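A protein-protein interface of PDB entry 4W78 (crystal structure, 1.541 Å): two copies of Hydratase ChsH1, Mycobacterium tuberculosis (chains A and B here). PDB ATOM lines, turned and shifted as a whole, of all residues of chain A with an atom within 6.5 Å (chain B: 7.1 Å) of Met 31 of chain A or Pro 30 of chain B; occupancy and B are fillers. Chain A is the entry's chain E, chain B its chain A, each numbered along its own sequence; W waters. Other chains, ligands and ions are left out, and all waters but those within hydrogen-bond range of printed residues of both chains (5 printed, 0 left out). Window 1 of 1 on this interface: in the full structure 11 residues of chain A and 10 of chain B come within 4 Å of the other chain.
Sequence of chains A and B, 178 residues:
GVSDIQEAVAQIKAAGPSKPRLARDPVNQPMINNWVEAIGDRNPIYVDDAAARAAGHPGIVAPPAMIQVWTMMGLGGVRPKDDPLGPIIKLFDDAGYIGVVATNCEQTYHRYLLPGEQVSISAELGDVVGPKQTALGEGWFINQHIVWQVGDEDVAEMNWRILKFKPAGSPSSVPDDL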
ATOM      1  N   ARG A  24      12.017 -14.747  -9.064  1.00  0.00           N
ATOM      2  CA  ARG A  24      10.592 -14.544  -8.831  1.00  0.00           C
ATOM      3  C   ARG A  24      10.046 -15.521  -7.794  1.00  0.00           C
ATOM      4  O   ARG A  24       9.250 -15.149  -6.932  1.00  0.00           O
ATOM      5  CB  ARG A  24       9.811 -14.700 -10.145  1.00  0.00           C
ATOM      6  CG  ARG A  24       8.333 -14.410 -10.000  1.00  0.00           C
ATOM      7  CD  ARG A  24       7.536 -14.784 -11.249  1.00  0.00           C
ATOM      8  NE  ARG A  24       7.518 -16.235 -11.390  1.00  0.00           N
ATOM      9  CZ  ARG A  24       6.941 -16.903 -12.378  1.00  0.00           C
ATOM     10  NH1 ARG A  24       6.340 -16.258 -13.358  1.00  0.00           N
ATOM     11  NH2 ARG A  24       6.999 -18.240 -12.376  1.00  0.00           N
ATOM     12  N   ASP A  25      10.493 -16.769  -7.893  1.00  0.00           N
ATOM     13  CA  ASP A  25      10.048 -17.822  -6.996  1.00  0.00           C
ATOM     14  C   ASP A  25      11.270 -18.460  -6.367  1.00  0.00           C
ATOM     15  O   ASP A  25      12.345 -18.460  -6.969  1.00  0.00           O
ATOM     16  CB  ASP A  25       9.286 -18.913  -7.769  1.00  0.00           C
ATOM     17  CG  ASP A  25       8.330 -18.348  -8.798  1.00  0.00           C
ATOM     18  OD1 ASP A  25       7.242 -17.877  -8.405  1.00  0.00           O
ATOM     19  OD2 ASP A  25       8.678 -18.362 -10.000  1.00  0.00           O
ATOM     20  N   PRO A  26      11.112 -19.024  -5.165  1.00  0.00           N
ATOM     21  CA  PRO A  26      12.123 -19.966  -4.679  1.00  0.00           C
ATOM     22  C   PRO A  26      12.149 -21.164  -5.619  1.00  0.00           C
ATOM     23  O   PRO A  26      11.213 -21.374  -6.387  1.00  0.00           O
ATOM     24  CB  PRO A  26      11.573 -20.421  -3.317  1.00  0.00           C
ATOM     25  CG  PRO A  26      10.461 -19.485  -2.984  1.00  0.00           C
ATOM     26  CD  PRO A  26       9.942 -18.946  -4.277  1.00  0.00           C
ATOM     27  N   ASN A  28      11.341 -24.564  -6.839  1.00  0.00           N
ATOM     28  CA  ASN A  28      10.057 -25.192  -6.527  1.00  0.00           C
ATOM     29  C   ASN A  28       9.712 -26.367  -7.419  1.00  0.00           C
ATOM     30  O   ASN A  28      10.113 -26.419  -8.587  1.00  0.00           O
ATOM     31  CB  ASN A  28       8.932 -24.151  -6.582  1.00  0.00           C
ATOM     32  CG  ASN A  28       8.724 -23.603  -7.973  1.00  0.00           C
ATOM     33  OD1 ASN A  28       7.980 -24.166  -8.766  1.00  0.00           O
ATOM     34  ND2 ASN A  28       9.400 -22.496  -8.285  1.00  0.00           N
ATOM     35  N   GLN A  29       8.971 -27.313  -6.843  1.00  0.00           N
ATOM     36  CA  GLN A  29       8.615 -28.531  -7.559  1.00  0.00           C
ATOM     37  C   GLN A  29       7.745 -28.326  -8.813  1.00  0.00           C
ATOM     38  O   GLN A  29       7.990 -28.971  -9.832  1.00  0.00           O
ATOM     39  CB  GLN A  29       7.960 -29.530  -6.614  1.00  0.00           C
ATOM     40  CG  GLN A  29       7.904 -30.922  -7.208  1.00  0.00           C
ATOM     41  CD  GLN A  29       9.286 -31.479  -7.383  1.00  0.00           C
ATOM     42  OE1 GLN A  29      10.106 -31.377  -6.473  1.00  0.00           O
ATOM     43  NE2 GLN A  29       9.562 -32.076  -8.533  1.00  0.00           N
ATOM     44  N   PRO A  30       6.750 -27.421  -8.757  1.00  0.00           N
ATOM     45  CA  PRO A  30       5.938 -27.252  -9.969  1.00  0.00           C
ATOM     46  C   PRO A  30       6.778 -26.855 -11.188  1.00  0.00           C
ATOM     47  O   PRO A  30       6.598 -27.395 -12.299  1.00  0.00           O
ATOM     48  CB  PRO A  30       4.934 -26.154  -9.559  1.00  0.00           C
ATOM     49  CG  PRO A  30       4.787 -26.330  -8.090  1.00  0.00           C
ATOM     50  CD  PRO A  30       6.183 -26.686  -7.610  1.00  0.00           C
ATOM     51  N   MET A  31       7.725 -25.933 -11.009  1.00  0.00           N
ATOM     52  CA  MET A  31       8.592 -25.560 -12.118  1.00  0.00           C
ATOM     53  C   MET A  31       9.590 -26.640 -12.509  1.00  0.00           C
ATOM     54  O   MET A  31       9.899 -26.801 -13.683  1.00  0.00           O
ATOM     55  CB  MET A  31       9.283 -24.233 -11.846  1.00  0.00           C
ATOM     56  CG  MET A  31       8.294 -23.081 -11.938  1.00  0.00           C
ATOM     57  SD  MET A  31       9.012 -21.479 -11.565  1.00  0.00           S
ATOM     58  CE  MET A  31      10.492 -21.500 -12.566  1.00  0.00           C
ATOM     59  N   ILE A  32      10.101 -27.381 -11.526  1.00  0.00           N
ATOM     60  CA  ILE A  32      10.914 -28.546 -11.859  1.00  0.00           C
ATOM     61  C   ILE A  32      10.088 -29.502 -12.699  1.00  0.00           C
ATOM     62  O   ILE A  32      10.551 -30.022 -13.726  1.00  0.00           O
ATOM     63  CB  ILE A  32      11.401 -29.257 -10.594  1.00  0.00           C
ATOM     64  CG1 ILE A  32      12.412 -28.368  -9.864  1.00  0.00           C
ATOM     65  CG2 ILE A  32      11.998 -30.605 -10.967  1.00  0.00           C
ATOM     66  CD1 ILE A  32      12.808 -28.895  -8.469  1.00  0.00           C
ATOM     67  N   ASN A  33       8.856 -29.751 -12.272  1.00  0.00           N
ATOM     68  CA  ASN A  33       7.988 -30.657 -13.010  1.00  0.00           C
ATOM     69  C   ASN A  33       7.778 -30.210 -14.447  1.00  0.00           C
ATOM     70  O   ASN A  33       7.861 -31.018 -15.363  1.00  0.00           O
ATOM     71  CB  ASN A  33       6.635 -30.805 -12.310  1.00  0.00           C
ATOM     72  CG  ASN A  33       6.715 -31.623 -11.037  1.00  0.00           C
ATOM     73  OD1 ASN A  33       7.657 -32.388 -10.824  1.00  0.00           O
ATOM     74  ND2 ASN A  33       5.696 -31.492 -10.201  1.00  0.00           N
ATOM     75  N   ASN A  34       7.528 -28.915 -14.642  1.00  0.00           N
ATOM     76  CA  ASN A  34       7.325 -28.422 -16.005  1.00  0.00           C
ATOM     77  C   ASN A  34       8.571 -28.655 -16.860  1.00  0.00           C
ATOM     78  O   ASN A  34       8.487 -29.012 -18.052  1.00  0.00           O
ATOM     79  CB  ASN A  34       7.014 -26.924 -15.973  1.00  0.00           C
ATOM     80  CG  ASN A  34       5.617 -26.611 -15.469  1.00  0.00           C
ATOM     81  OD1 ASN A  34       4.750 -27.476 -15.378  1.00  0.00           O
ATOM     82  ND2 ASN A  34       5.385 -25.328 -15.169  1.00  0.00           N
ATOM     83  N   TRP A  35       9.728 -28.419 -16.256  1.00  0.00           N
ATOM     84  CA  TRP A  35      10.989 -28.496 -16.973  1.00  0.00           C
ATOM     85  C   TRP A  35      11.344 -29.937 -17.304  1.00  0.00           C
ATOM     86  O   TRP A  35      11.681 -30.242 -18.442  1.00  0.00           O
ATOM     87  CB  TRP A  35      12.068 -27.827 -16.129  1.00  0.00           C
ATOM     88  CG  TRP A  35      13.407 -27.609 -16.767  1.00  0.00           C
ATOM     89  CD1 TRP A  35      13.847 -26.457 -17.344  1.00  0.00           C
ATOM     90  CD2 TRP A  35      14.505 -28.533 -16.823  1.00  0.00           C
ATOM     91  NE1 TRP A  35      15.141 -26.601 -17.762  1.00  0.00           N
ATOM     92  CE2 TRP A  35      15.565 -27.866 -17.470  1.00  0.00           C
ATOM     93  CE3 TRP A  35      14.688 -29.848 -16.400  1.00  0.00           C
ATOM     94  CZ2 TRP A  35      16.801 -28.464 -17.699  1.00  0.00           C
ATOM     95  CZ3 TRP A  35      15.929 -30.452 -16.634  1.00  0.00           C
ATOM     96  CH2 TRP A  35      16.959 -29.749 -17.292  1.00  0.00           C
ATOM     97  N   VAL A  36      11.279 -30.846 -16.330  1.00  0.00           N
ATOM     98  CA  VAL A  36      11.647 -32.229 -16.648  1.00  0.00           C
ATOM     99  C   VAL A  36      10.668 -32.860 -17.650  1.00  0.00           C
ATOM    100  O   VAL A  36      11.054 -33.692 -18.485  1.00  0.00           O
ATOM    101  CB  VAL A  36      11.832 -33.122 -15.380  1.00  0.00           C
ATOM    102  CG1 VAL A  36      12.929 -32.548 -14.483  1.00  0.00           C
ATOM    103  CG2 VAL A  36      10.518 -33.316 -14.646  1.00  0.00           C
ATOM    104  N   MET A  66      18.785 -26.002 -14.522  1.00  0.00           N
ATOM    105  CA  MET A  66      17.691 -25.048 -14.308  1.00  0.00           C
ATOM    106  C   MET A  66      18.125 -23.726 -13.677  1.00  0.00           C
ATOM    107  O   MET A  66      17.280 -22.860 -13.448  1.00  0.00           O
ATOM    108  CB  MET A  66      16.591 -25.651 -13.431  1.00  0.00           C
ATOM    109  CG  MET A  66      15.669 -26.603 -14.168  1.00  0.00           C
ATOM    110  SD  MET A  66      14.202 -26.993 -13.212  1.00  0.00           S
ATOM    111  CE  MET A  66      13.236 -25.503 -13.512  1.00  0.00           C
ATOM    112  N   VAL A  69      16.866 -20.632 -15.198  1.00  0.00           N
ATOM    113  CA  VAL A  69      15.415 -20.581 -15.266  1.00  0.00           C
ATOM    114  C   VAL A  69      14.818 -19.773 -14.111  1.00  0.00           C
ATOM    115  O   VAL A  69      13.852 -19.028 -14.300  1.00  0.00           O
ATOM    116  CB  VAL A  69      14.815 -22.009 -15.305  1.00  0.00           C
ATOM    117  CG1 VAL A  69      13.295 -21.950 -15.435  1.00  0.00           C
ATOM    118  CG2 VAL A  69      15.387 -22.790 -16.482  1.00  0.00           C
ATOM    119  N   TRP A  70      15.389 -19.921 -12.913  1.00  0.00           N
ATOM    120  CA  TRP A  70      14.778 -19.310 -11.742  1.00  0.00           C
ATOM    121  C   TRP A  70      14.736 -17.800 -11.841  1.00  0.00           C
ATOM    122  O   TRP A  70      13.800 -17.157 -11.347  1.00  0.00           O
ATOM    123  CB  TRP A  70      15.506 -19.715 -10.446  1.00  0.00           C
ATOM    124  CG  TRP A  70      15.637 -21.206 -10.306  1.00  0.00           C
ATOM    125  CD1 TRP A  70      16.792 -21.938 -10.339  1.00  0.00           C
ATOM    126  CD2 TRP A  70      14.561 -22.138 -10.176  1.00  0.00           C
ATOM    127  NE1 TRP A  70      16.503 -23.281 -10.223  1.00  0.00           N
ATOM    128  CE2 TRP A  70      15.140 -23.428 -10.128  1.00  0.00           C
ATOM    129  CE3 TRP A  70      13.165 -22.010 -10.124  1.00  0.00           C
ATOM    130  CZ2 TRP A  70      14.376 -24.578 -10.011  1.00  0.00           C
ATOM    131  CZ3 TRP A  70      12.391 -23.176 -10.000  1.00  0.00           C
ATOM    132  CH2 TRP A  70      13.014 -24.444  -9.942  1.00  0.00           C
ATOM    133  N   ARG B  24      -1.411 -32.827 -10.310  1.00  0.00           N
ATOM    134  CA  ARG B  24       0.032 -33.052 -10.259  1.00  0.00           C
ATOM    135  C   ARG B  24       0.684 -32.294  -9.101  1.00  0.00           C
ATOM    136  O   ARG B  24       1.559 -32.826  -8.408  1.00  0.00           O
ATOM    137  CB  ARG B  24       0.683 -32.636 -11.585  1.00  0.00           C
ATOM    138  CG  ARG B  24       2.159 -32.956 -11.642  1.00  0.00           C
ATOM    139  CD  ARG B  24       2.837 -32.297 -12.840  1.00  0.00           C
ATOM    140  NE  ARG B  24       2.908 -30.853 -12.667  1.00  0.00           N
ATOM    141  CZ  ARG B  24       3.452 -30.005 -13.535  1.00  0.00           C
ATOM    142  NH1 ARG B  24       3.996 -30.444 -14.664  1.00  0.00           N
ATOM    143  NH2 ARG B  24       3.450 -28.712 -13.248  1.00  0.00           N
ATOM    144  N   ASP B  25       0.269 -31.045  -8.914  1.00  0.00           N
ATOM    145  CA  ASP B  25       0.819 -30.184  -7.866  1.00  0.00           C
ATOM    146  C   ASP B  25      -0.308 -29.656  -7.004  1.00  0.00           C
ATOM    147  O   ASP B  25      -1.434 -29.507  -7.470  1.00  0.00           O
ATOM    148  CB  ASP B  25       1.523 -28.954  -8.478  1.00  0.00           C
ATOM    149  CG  ASP B  25       2.346 -29.287  -9.707  1.00  0.00           C
ATOM    150  OD1 ASP B  25       3.449 -29.829  -9.541  1.00  0.00           O
ATOM    151  OD2 ASP B  25       1.880 -29.008 -10.832  1.00  0.00           O
ATOM    152  N   VAL B  27      -2.157 -26.417  -5.411  1.00  0.00           N
ATOM    153  CA  VAL B  27      -2.245 -25.013  -5.825  1.00  0.00           C
ATOM    154  C   VAL B  27      -0.949 -24.346  -5.386  1.00  0.00           C
ATOM    155  O   VAL B  27      -0.469 -24.577  -4.263  1.00  0.00           O
ATOM    156  CB  VAL B  27      -3.450 -24.340  -5.151  1.00  0.00           C
ATOM    157  CG1 VAL B  27      -3.491 -22.832  -5.464  1.00  0.00           C
ATOM    158  CG2 VAL B  27      -4.749 -25.040  -5.588  1.00  0.00           C
ATOM    159  N   ASN B  28      -0.342 -23.557  -6.271  1.00  0.00           N
ATOM    160  CA  ASN B  28       0.984 -23.030  -5.964  1.00  0.00           C
ATOM    161  C   ASN B  28       1.256 -21.695  -6.635  1.00  0.00           C
ATOM    162  O   ASN B  28       0.762 -21.434  -7.735  1.00  0.00           O
ATOM    163  CB  ASN B  28       2.071 -24.048  -6.340  1.00  0.00           C
ATOM    164  CG  ASN B  28       2.150 -24.292  -7.816  1.00  0.00           C
ATOM    165  OD1 ASN B  28       2.868 -23.593  -8.530  1.00  0.00           O
ATOM    166  ND2 ASN B  28       1.430 -25.308  -8.288  1.00  0.00           N
ATOM    167  N   GLN B  29       2.034 -20.865  -5.950  1.00  0.00           N
ATOM    168  CA  GLN B  29       2.349 -19.526  -6.431  1.00  0.00           C
ATOM    169  C   GLN B  29       3.078 -19.476  -7.793  1.00  0.00           C
ATOM    170  O   GLN B  29       2.737 -18.625  -8.612  1.00  0.00           O
ATOM    171  CB  GLN B  29       3.105 -18.713  -5.367  1.00  0.00           C
ATOM    172  CG  GLN B  29       3.106 -17.218  -5.688  1.00  0.00           C
ATOM    173  CD  GLN B  29       1.707 -16.631  -5.588  1.00  0.00           C
ATOM    174  OE1 GLN B  29       1.001 -16.900  -4.615  1.00  0.00           O
ATOM    175  NE2 GLN B  29       1.296 -15.838  -6.591  1.00  0.00           N
ATOM    176  N   PRO B  30       4.077 -20.357  -8.039  1.00  0.00           N
ATOM    177  CA  PRO B  30       4.767 -20.271  -9.333  1.00  0.00           C
ATOM    178  C   PRO B  30       3.819 -20.434 -10.514  1.00  0.00           C
ATOM    179  O   PRO B  30       3.928 -19.674 -11.487  1.00  0.00           O
ATOM    180  CB  PRO B  30       5.800 -21.412  -9.264  1.00  0.00           C
ATOM    181  CG  PRO B  30       6.109 -21.501  -7.784  1.00  0.00           C
ATOM    182  CD  PRO B  30       4.753 -21.310  -7.129  1.00  0.00           C
ATOM    183  N   MET B  31       2.878 -21.366 -10.421  1.00  0.00           N
ATOM    184  CA  MET B  31       1.906 -21.532 -11.504  1.00  0.00           C
ATOM    185  C   MET B  31       0.851 -20.425 -11.559  1.00  0.00           C
ATOM    186  O   MET B  31       0.439 -20.051 -12.642  1.00  0.00           O
ATOM    187  CB  MET B  31       1.259 -22.908 -11.437  1.00  0.00           C
ATOM    188  CG  MET B  31       2.227 -23.979 -11.822  1.00  0.00           C
ATOM    189  SD  MET B  31       1.579 -25.647 -11.730  1.00  0.00           S
ATOM    190  CE  MET B  31       0.030 -25.474 -12.618  1.00  0.00           C
ATOM    191  N   ILE B  32       0.443 -19.881 -10.417  1.00  0.00           N
ATOM    192  CA  ILE B  32      -0.405 -18.703 -10.408  1.00  0.00           C
ATOM    193  C   ILE B  32       0.326 -17.569 -11.117  1.00  0.00           C
ATOM    194  O   ILE B  32      -0.271 -16.865 -11.950  1.00  0.00           O
ATOM    195  CB  ILE B  32      -0.759 -18.268  -8.977  1.00  0.00           C
ATOM    196  CG1 ILE B  32      -1.667 -19.322  -8.316  1.00  0.00           C
ATOM    197  CG2 ILE B  32      -1.420 -16.879  -8.982  1.00  0.00           C
ATOM    198  CD1 ILE B  32      -1.910 -19.048  -6.846  1.00  0.00           C
ATOM    199  N   ASN B  33       1.609 -17.402 -10.795  1.00  0.00           N
ATOM    200  CA  ASN B  33       2.411 -16.353 -11.428  1.00  0.00           C
ATOM    201  C   ASN B  33       2.454 -16.506 -12.941  1.00  0.00           C
ATOM    202  O   ASN B  33       2.270 -15.529 -13.665  1.00  0.00           O
ATOM    203  CB  ASN B  33       3.836 -16.318 -10.866  1.00  0.00           C
ATOM    204  CG  ASN B  33       3.908 -15.738  -9.447  1.00  0.00           C
ATOM    205  OD1 ASN B  33       2.989 -15.062  -8.996  1.00  0.00           O
ATOM    206  ND2 ASN B  33       5.018 -15.975  -8.758  1.00  0.00           N
ATOM    207  N   ASN B  34       2.699 -17.723 -13.422  1.00  0.00           N
ATOM    208  CA  ASN B  34       2.779 -17.944 -14.859  1.00  0.00           C
ATOM    209  C   ASN B  34       1.459 -17.567 -15.519  1.00  0.00           C
ATOM    210  O   ASN B  34       1.436 -16.980 -16.605  1.00  0.00           O
ATOM    211  CB  ASN B  34       3.117 -19.405 -15.174  1.00  0.00           C
ATOM    212  CG  ASN B  34       4.564 -19.775 -14.834  1.00  0.00           C
ATOM    213  OD1 ASN B  34       5.424 -18.914 -14.672  1.00  0.00           O
ATOM    214  ND2 ASN B  34       4.825 -21.070 -14.753  1.00  0.00           N
ATOM    215  N   TRP B  35       0.364 -17.925 -14.857  1.00  0.00           N
ATOM    216  CA  TRP B  35      -0.979 -17.724 -15.392  1.00  0.00           C
ATOM    217  C   TRP B  35      -1.376 -16.251 -15.391  1.00  0.00           C
ATOM    218  O   TRP B  35      -1.781 -15.724 -16.436  1.00  0.00           O
ATOM    219  CB  TRP B  35      -1.962 -18.592 -14.601  1.00  0.00           C
ATOM    220  CG  TRP B  35      -3.354 -18.741 -15.150  1.00  0.00           C
ATOM    221  CD1 TRP B  35      -3.842 -19.785 -15.875  1.00  0.00           C
ATOM    222  CD2 TRP B  35      -4.450 -17.840 -14.950  1.00  0.00           C
ATOM    223  NE1 TRP B  35      -5.186 -19.586 -16.153  1.00  0.00           N
ATOM    224  CE2 TRP B  35      -5.576 -18.398 -15.595  1.00  0.00           C
ATOM    225  CE3 TRP B  35      -4.590 -16.630 -14.269  1.00  0.00           C
ATOM    226  CZ2 TRP B  35      -6.818 -17.778 -15.593  1.00  0.00           C
ATOM    227  CZ3 TRP B  35      -5.839 -15.994 -14.286  1.00  0.00           C
ATOM    228  CH2 TRP B  35      -6.926 -16.570 -14.950  1.00  0.00           C
ATOM    229  N   GLU B  37       0.486 -13.673 -15.368  1.00  0.00           N
ATOM    230  CA  GLU B  37       1.351 -12.938 -16.276  1.00  0.00           C
ATOM    231  C   GLU B  37       0.913 -13.117 -17.733  1.00  0.00           C
ATOM    232  O   GLU B  37       0.904 -12.148 -18.502  1.00  0.00           O
ATOM    233  CB  GLU B  37       2.813 -13.351 -16.094  1.00  0.00           C
ATOM    234  CG  GLU B  37       3.386 -12.871 -14.757  1.00  0.00           C
ATOM    235  CD  GLU B  37       4.772 -13.419 -14.472  1.00  0.00           C
ATOM    236  OE1 GLU B  37       5.477 -13.798 -15.433  1.00  0.00           O
ATOM    237  OE2 GLU B  37       5.148 -13.469 -13.278  1.00  0.00           O
ATOM    238  N   MET B  66      -8.509 -20.737 -12.709  1.00  0.00           N
ATOM    239  CA  MET B  66      -7.433 -21.736 -12.777  1.00  0.00           C
ATOM    240  C   MET B  66      -7.832 -23.148 -12.351  1.00  0.00           C
ATOM    241  O   MET B  66      -6.997 -24.058 -12.418  1.00  0.00           O
ATOM    242  CB  MET B  66      -6.214 -21.303 -11.942  1.00  0.00           C
ATOM    243  CG  MET B  66      -5.379 -20.216 -12.592  1.00  0.00           C
ATOM    244  SD  MET B  66      -3.788 -20.010 -11.756  1.00  0.00           S
ATOM    245  CE  MET B  66      -2.868 -21.408 -12.401  1.00  0.00           C
ATOM    246  N   TRP B  70      -5.121 -26.980 -12.654  1.00  0.00           N
ATOM    247  CA  TRP B  70      -4.423 -27.815 -11.684  1.00  0.00           C
ATOM    248  C   TRP B  70      -4.447 -29.273 -12.082  1.00  0.00           C
ATOM    249  O   TRP B  70      -3.465 -30.000 -11.852  1.00  0.00           O
ATOM    250  CB  TRP B  70      -5.023 -27.637 -10.282  1.00  0.00           C
ATOM    251  CG  TRP B  70      -5.048 -26.205  -9.862  1.00  0.00           C
ATOM    252  CD1 TRP B  70      -6.154 -25.454  -9.600  1.00  0.00           C
ATOM    253  CD2 TRP B  70      -3.921 -25.328  -9.711  1.00  0.00           C
ATOM    254  NE1 TRP B  70      -5.788 -24.165  -9.282  1.00  0.00           N
ATOM    255  CE2 TRP B  70      -4.426 -24.066  -9.337  1.00  0.00           C
ATOM    256  CE3 TRP B  70      -2.537 -25.491  -9.845  1.00  0.00           C
ATOM    257  CZ2 TRP B  70      -3.600 -22.971  -9.112  1.00  0.00           C
ATOM    258  CZ3 TRP B  70      -1.714 -24.400  -9.623  1.00  0.00           C
ATOM    259  CH2 TRP B  70      -2.254 -23.156  -9.252  1.00  0.00           C
HETATM  260  O   HOH W   1       7.287 -23.120 -15.469  1.00  0.00           O
HETATM  261  O   HOH W   2       7.361 -17.532 -16.362  1.00  0.00           O
HETATM  262  O   HOH W   3       8.065 -13.949 -15.114  1.00  0.00           O
HETATM  263  O   HOH W   4       6.061 -14.928  -6.134  1.00  0.00           O
HETATM  264  O   HOH W   5       2.856 -23.264 -15.400  1.00  0.00           O
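OD1 of Asn 34 of chain A is in hydrogen-bond range of NH2 of Arg 24 of chain B, at 2.8 Å. ND2 of Asn 33 of chain A is in hydrogen-bond range of OD1 of Asp 25 of chain B (2.9 Å). The side-chain amide nitrogen of Asn 33 of chain B sits at hydrogen-bond distance from the side-chain carboxylate of Asp 25 of chain A, at 2.9 Å. The side-chain amide oxygen (OD1) of Asn 34 of chain B lies within hydrogen-bond range of the guanidinium group (NH2) of Arg 24 of chain A. The guanidinium group (NH1) of Arg 24 of chain A is in salt-bridge range of the side-chain carboxylate (OE2) of Glu 37 of chain B, 3.0 Å away.
NE of Arg 24 of chain B is in salt-bridge range of OD2 of Asp 25 of chain B (2.8 Å). OD1 of Asn 28 of chain B is in hydrogen-bond range of N of Met 31 of chain B. The side-chain amide oxygen (OD1) of Asn 33 of chain B lies within hydrogen-bond range of the side-chain amide nitrogen (NE2) of Gln 29 of chain B. The guanidinium group (NE) of Arg 24 of chain A lies within salt-bridge range of the side-chain carboxylate (OD2) of Asp 25 of chain A, 2.8 Å away. O of Pro 26 of chain A is in hydrogen-bond range of ND2 of Asn 28 of chain A, 2.9 Å away. The side-chain amide oxygen of Asn 28 of chain A sits at hydrogen-bond distance from the backbone NH of Met 31 of chain A.
Among the printed residues, merely in contact across the chains: Arg 24 of chain A with Pro 30 of chain B, Arg 24 of chain A with Asn 33 of chain B, Asp 25 of chain A with Pro 30 of chain B, Asn 28 of chain A with Pro 30 of chain B, Pro 30 of chain A with Arg 24 of chain B, Pro 30 of chain A with Asp 25 of chain B, Pro 30 of chain A with Asn 28 of chain B, Met 31 of chain A with Pro 30 of chain B and Asn 33 of chain A with Arg 24 of chain B.
Of the printed residues of chain B, Pro 30 of chain A touches Arg 24, Asp 25 and Asn 28. Of chain B, only Pro 30 (3.95 Å) comes within 4 Å of Met 31 of chain A. Printed residues of chain B within 4 Å of Asn 34 of chain A: Arg 24 (2.8 Å). Trp 35 of chain A touches none of the printed residues of chain B. Of the printed residues of chain A, Asn 28 of chain B touches Pro 30. Pro 30 of chain B touches just these residues of chain A: Arg 24 (3.5 Å), Asp 25 (3.6 Å), Asn 28 (3.4 Å) and Met 31 (3.95 Å). Of the printed residues of chain A, Asn 34 of chain B touches Arg 24 (2.9 Å). Of the printed residues of chain A, Glu 37 of chain B touches Arg 24 (3.0 Å). The nearest residue of chain B that does not touch Met 31 of chain A is Asn 34 of chain B (4.9 Å). The nearest printed residue of chain B that does not touch Asn 33 of chain A is Met 31 of chain B (7.2 Å).
Printed residues of chain A that touch a printed residue of chain B: Arg 24, Asp 25, Asn 28, Pro 30, Met 31, Asn 33 and Asn 34. Hydrophobic or aromatic side chains of chain A that line the printed part of chain B: Pro 30 and Met 31. Among the printed residues, 14 pairs touch across the chains. Among the printed residues, Asp or Glu carboxylates within 4 Å of a Lys or Arg side-chain nitrogen of the other chain: Arg 24 of chain A with Glu 37 of chain B (3.0 Å).
Arg 24 of chain A touches Pro 30 of chain B, and with the chains exchanged Pro 30 of chain A touches Arg 24 of chain B. Arg 24 of chain A touches Asn 33 of chain B, and with the chains exchanged Asn 33 of chain A touches Arg 24 of chain B. Arg 24 of chain A touches Asn 34 of chain B, and with the chains exchanged Asn 34 of chain A touches Arg 24 of chain B. Asp 25 of chain A touches Pro 30 of chain B, and with the chains exchanged Pro 30 of chain A touches Asp 25 of chain B. Positions printed for both chains: 24, 25, 28, 29, 30, 31, 32, 33, 34, 35, 66 and 70. Of the 14 pairs that touch across the chains among the printed residues, 12 have their exchanged pair printed and touching as well.
Water W3 bridges the side-chain carboxylate of Glu 37 of chain B (2.6 Å) and the guanidinium group of Arg 24 of chain A (3.4 Å). Water W2 bridges OD1 of Asn 34 of chain B (2.9 Å) and NH1 of Arg 24 of chain A (3.4 Å). Water W1 bridges ND2 of Asn 34 of chain A (2.9 Å) and ND2 of Asn 34 of chain B (3.3 Å). Water W4 bridges the side-chain amide nitrogen (ND2) of Asn 33 of chain B and the backbone carbonyl oxygen (O) of Arg 24 of chain A. Water W5 lies within hydrogen-bond range of the side-chain amide nitrogen of Asn 34 of chain B (3.0 Å) and the side-chain amide nitrogen of Asn 34 of chain A (3.3 Å).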
